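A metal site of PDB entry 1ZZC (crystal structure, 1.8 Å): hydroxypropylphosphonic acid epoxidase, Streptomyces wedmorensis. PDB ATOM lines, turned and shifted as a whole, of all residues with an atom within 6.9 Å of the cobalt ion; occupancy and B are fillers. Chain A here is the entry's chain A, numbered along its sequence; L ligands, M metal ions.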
ATOM      1  N   ASN A 135     -11.422   5.537 -11.722  1.00  0.00           N
ATOM      2  CA  ASN A 135     -11.127   4.818 -12.946  1.00  0.00           C
ATOM      3  C   ASN A 135      -9.934   3.923 -12.570  1.00  0.00           C
ATOM      4  O   ASN A 135      -8.911   4.420 -12.080  1.00  0.00           O
ATOM      5  CB  ASN A 135     -10.695   5.842 -14.017  1.00  0.00           C
ATOM      6  CG  ASN A 135     -10.398   5.186 -15.337  1.00  0.00           C
ATOM      7  OD1 ASN A 135      -9.466   4.401 -15.434  1.00  0.00           O
ATOM      8  ND2 ASN A 135     -11.223   5.444 -16.351  1.00  0.00           N
ATOM      9  N   GLY A 137      -7.532   2.925 -13.827  1.00  0.00           N
ATOM     10  CA  GLY A 137      -6.256   3.183 -14.468  1.00  0.00           C
ATOM     11  C   GLY A 137      -6.353   2.942 -15.961  1.00  0.00           C
ATOM     12  O   GLY A 137      -7.213   2.191 -16.434  1.00  0.00           O
ATOM     13  N   HIS A 138      -5.467   3.561 -16.736  1.00  0.00           N
ATOM     14  CA  HIS A 138      -5.499   3.401 -18.176  1.00  0.00           C
ATOM     15  C   HIS A 138      -4.297   2.718 -18.757  1.00  0.00           C
ATOM     16  O   HIS A 138      -3.220   2.683 -18.157  1.00  0.00           O
ATOM     17  CB  HIS A 138      -5.520   4.759 -18.896  1.00  0.00           C
ATOM     18  CG  HIS A 138      -6.649   5.650 -18.500  1.00  0.00           C
ATOM     19  ND1 HIS A 138      -7.957   5.222 -18.461  1.00  0.00           N
ATOM     20  CD2 HIS A 138      -6.668   6.961 -18.152  1.00  0.00           C
ATOM     21  CE1 HIS A 138      -8.728   6.230 -18.109  1.00  0.00           C
ATOM     22  NE2 HIS A 138      -7.972   7.298 -17.916  1.00  0.00           N
ATOM     23  N   GLU A 142      -2.040  10.224 -19.700  1.00  0.00           N
ATOM     24  CA  GLU A 142      -3.109  11.204 -19.794  1.00  0.00           C
ATOM     25  C   GLU A 142      -2.644  12.584 -19.345  1.00  0.00           C
ATOM     26  O   GLU A 142      -1.932  12.717 -18.355  1.00  0.00           O
ATOM     27  CB  GLU A 142      -4.320  10.771 -18.949  1.00  0.00           C
ATOM     28  CG  GLU A 142      -5.499  11.749 -19.031  1.00  0.00           C
ATOM     29  CD  GLU A 142      -6.757  11.247 -18.300  1.00  0.00           C
ATOM     30  OE1 GLU A 142      -7.675  12.066 -18.051  1.00  0.00           O
ATOM     31  OE2 GLU A 142      -6.832  10.044 -17.983  1.00  0.00           O
ATOM     32  N   LEU A 144      -4.157  16.510 -18.540  1.00  0.00           N
ATOM     33  CA  LEU A 144      -5.412  17.233 -18.234  1.00  0.00           C
ATOM     34  C   LEU A 144      -5.127  18.723 -18.039  1.00  0.00           C
ATOM     35  O   LEU A 144      -4.055  19.114 -17.560  1.00  0.00           O
ATOM     36  CB  LEU A 144      -6.087  16.686 -16.975  1.00  0.00           C
ATOM     37  CG  LEU A 144      -6.580  15.233 -16.914  1.00  0.00           C
ATOM     38  CD1 LEU A 144      -5.465  14.359 -16.351  1.00  0.00           C
ATOM     39  CD2 LEU A 144      -7.804  15.122 -15.991  1.00  0.00           C
ATOM     40  N   VAL A 174      -1.011  12.086 -15.725  1.00  0.00           N
ATOM     41  CA  VAL A 174      -1.299  10.860 -14.996  1.00  0.00           C
ATOM     42  C   VAL A 174      -0.758   9.724 -15.855  1.00  0.00           C
ATOM     43  O   VAL A 174      -1.172   9.528 -16.995  1.00  0.00           O
ATOM     44  CB  VAL A 174      -2.811  10.599 -14.797  1.00  0.00           C
ATOM     45  CG1 VAL A 174      -3.006   9.291 -14.005  1.00  0.00           C
ATOM     46  CG2 VAL A 174      -3.473  11.760 -14.053  1.00  0.00           C
ATOM     47  N   VAL A 178      -2.521   4.369 -13.401  1.00  0.00           N
ATOM     48  CA  VAL A 178      -2.801   5.029 -12.131  1.00  0.00           C
ATOM     49  C   VAL A 178      -4.295   5.336 -12.042  1.00  0.00           C
ATOM     50  O   VAL A 178      -4.847   6.031 -12.889  1.00  0.00           O
ATOM     51  CB  VAL A 178      -2.020   6.355 -11.988  1.00  0.00           C
ATOM     52  CG1 VAL A 178      -2.389   7.010 -10.656  1.00  0.00           C
ATOM     53  CG2 VAL A 178      -0.516   6.097 -12.072  1.00  0.00           C
ATOM     54  N   HIS A 180      -7.711   7.103 -11.052  1.00  0.00           N
ATOM     55  CA  HIS A 180      -8.005   8.495 -10.768  1.00  0.00           C
ATOM     56  C   HIS A 180      -9.499   8.798 -10.859  1.00  0.00           C
ATOM     57  O   HIS A 180     -10.258   8.043 -11.444  1.00  0.00           O
ATOM     58  CB  HIS A 180      -7.208   9.419 -11.717  1.00  0.00           C
ATOM     59  CG  HIS A 180      -7.375   9.088 -13.169  1.00  0.00           C
ATOM     60  ND1 HIS A 180      -6.794   7.983 -13.752  1.00  0.00           N
ATOM     61  CD2 HIS A 180      -8.089   9.702 -14.144  1.00  0.00           C
ATOM     62  CE1 HIS A 180      -7.133   7.932 -15.026  1.00  0.00           C
ATOM     63  NE2 HIS A 180      -7.920   8.958 -15.293  1.00  0.00           N
ATOM     64  N   PHE A 182     -12.419  12.473 -10.288  1.00  0.00           N
ATOM     65  CA  PHE A 182     -12.519  13.873  -9.948  1.00  0.00           C
ATOM     66  C   PHE A 182     -13.944  14.401  -9.987  1.00  0.00           C
ATOM     67  O   PHE A 182     -14.828  13.791 -10.599  1.00  0.00           O
ATOM     68  CB  PHE A 182     -11.652  14.709 -10.872  1.00  0.00           C
ATOM     69  CG  PHE A 182     -11.886  14.452 -12.323  1.00  0.00           C
ATOM     70  CD1 PHE A 182     -11.157  13.466 -12.991  1.00  0.00           C
ATOM     71  CD2 PHE A 182     -12.877  15.150 -13.015  1.00  0.00           C
ATOM     72  CE1 PHE A 182     -11.401  13.191 -14.328  1.00  0.00           C
ATOM     73  CE2 PHE A 182     -13.138  14.881 -14.352  1.00  0.00           C
ATOM     74  CZ  PHE A 182     -12.403  13.895 -15.028  1.00  0.00           C
ATOM     75  N   ALA A 195      -9.299  16.613 -21.270  1.00  0.00           N
ATOM     76  CA  ALA A 195      -8.510  15.448 -20.913  1.00  0.00           C
ATOM     77  C   ALA A 195      -8.014  14.858 -22.211  1.00  0.00           C
ATOM     78  O   ALA A 195      -8.793  14.593 -23.110  1.00  0.00           O
ATOM     79  CB  ALA A 195      -9.362  14.429 -20.165  1.00  0.00           C
ATOM     80  N   ASN A 197      -6.047  11.661 -23.575  1.00  0.00           N
ATOM     81  CA  ASN A 197      -5.432  10.370 -23.329  1.00  0.00           C
ATOM     82  C   ASN A 197      -4.617  10.069 -24.593  1.00  0.00           C
ATOM     83  O   ASN A 197      -5.072  10.345 -25.712  1.00  0.00           O
ATOM     84  CB  ASN A 197      -6.505   9.307 -23.072  1.00  0.00           C
ATOM     85  CG  ASN A 197      -7.042   9.361 -21.631  1.00  0.00           C
ATOM     86  OD1 ASN A 197      -6.682   8.541 -20.787  1.00  0.00           O
ATOM     87  ND2 ASN A 197      -7.873  10.350 -21.353  1.00  0.00           N
HETATM   88  C1  LIG L   1     -10.933  10.111 -18.234  1.00  0.00           C
HETATM   89  C2  LIG L   1     -11.503   9.108 -17.230  1.00  0.00           C
HETATM   90  C3  LIG L   1     -10.392  11.351 -17.505  1.00  0.00           C
HETATM   91  C4  LIG L   1     -12.046  10.540 -19.203  1.00  0.00           C
HETATM   92  N1  LIG L   1      -9.846   9.466 -19.011  1.00  0.00           N
HETATM   93  O1  LIG L   1     -10.452   8.278 -16.745  1.00  0.00           O
HETATM   94  O2  LIG L   1      -9.537  10.948 -16.419  1.00  0.00           O
HETATM   95  O3  LIG L   1     -12.482   9.407 -19.961  1.00  0.00           O
HETATM   96 CO    CO M   1      -8.535   9.117 -17.221  1.00  0.00          CO
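O of Glu 142 sits at hydrogen-bond distance from N of Val 174, 2.9 Å away.
A ring nitrogen (ND1) of His 138 sits close to the side-chain amide oxygen (OD1) of Asn 135 (3.5 Å).
ND1 of His 180 is in hydrogen-bond range of O of Val 178 (2.9 Å).
A ring nitrogen (NE2) of His 138 sits close to the side-chain amide oxygen (OD1) of Asn 197 (3.4 Å).
The backbone NH (N) of Asn 135 is in hydrogen-bond range of the backbone carbonyl oxygen (O) of His 180, 2.8 Å away.
The side-chain carboxylate (OE2) of Glu 142 lies close to the side-chain amide oxygen (OD1) of Asn 197, at 3.2 Å.
Three residues have an atom within 4 Å of the cobalt ion: His 138, Glu 142 and His 180.
The nearest printed residue that does not touch the cobalt ion is Asn 197 (4.1 Å).
NE2 of His 138 is bound to the cobalt ion (2.0 Å).
NE2 of His 180 binds the cobalt ion, at 2.0 Å.
The cobalt ion is bound by OE2 of Glu 142, at 2.1 Å.
An oxygen (O1) of the ligand binds the cobalt ion.
O2 of the ligand binds the cobalt ion.
A nitrogen (N1) of the ligand binds the cobalt ion, 2.2 Å away.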
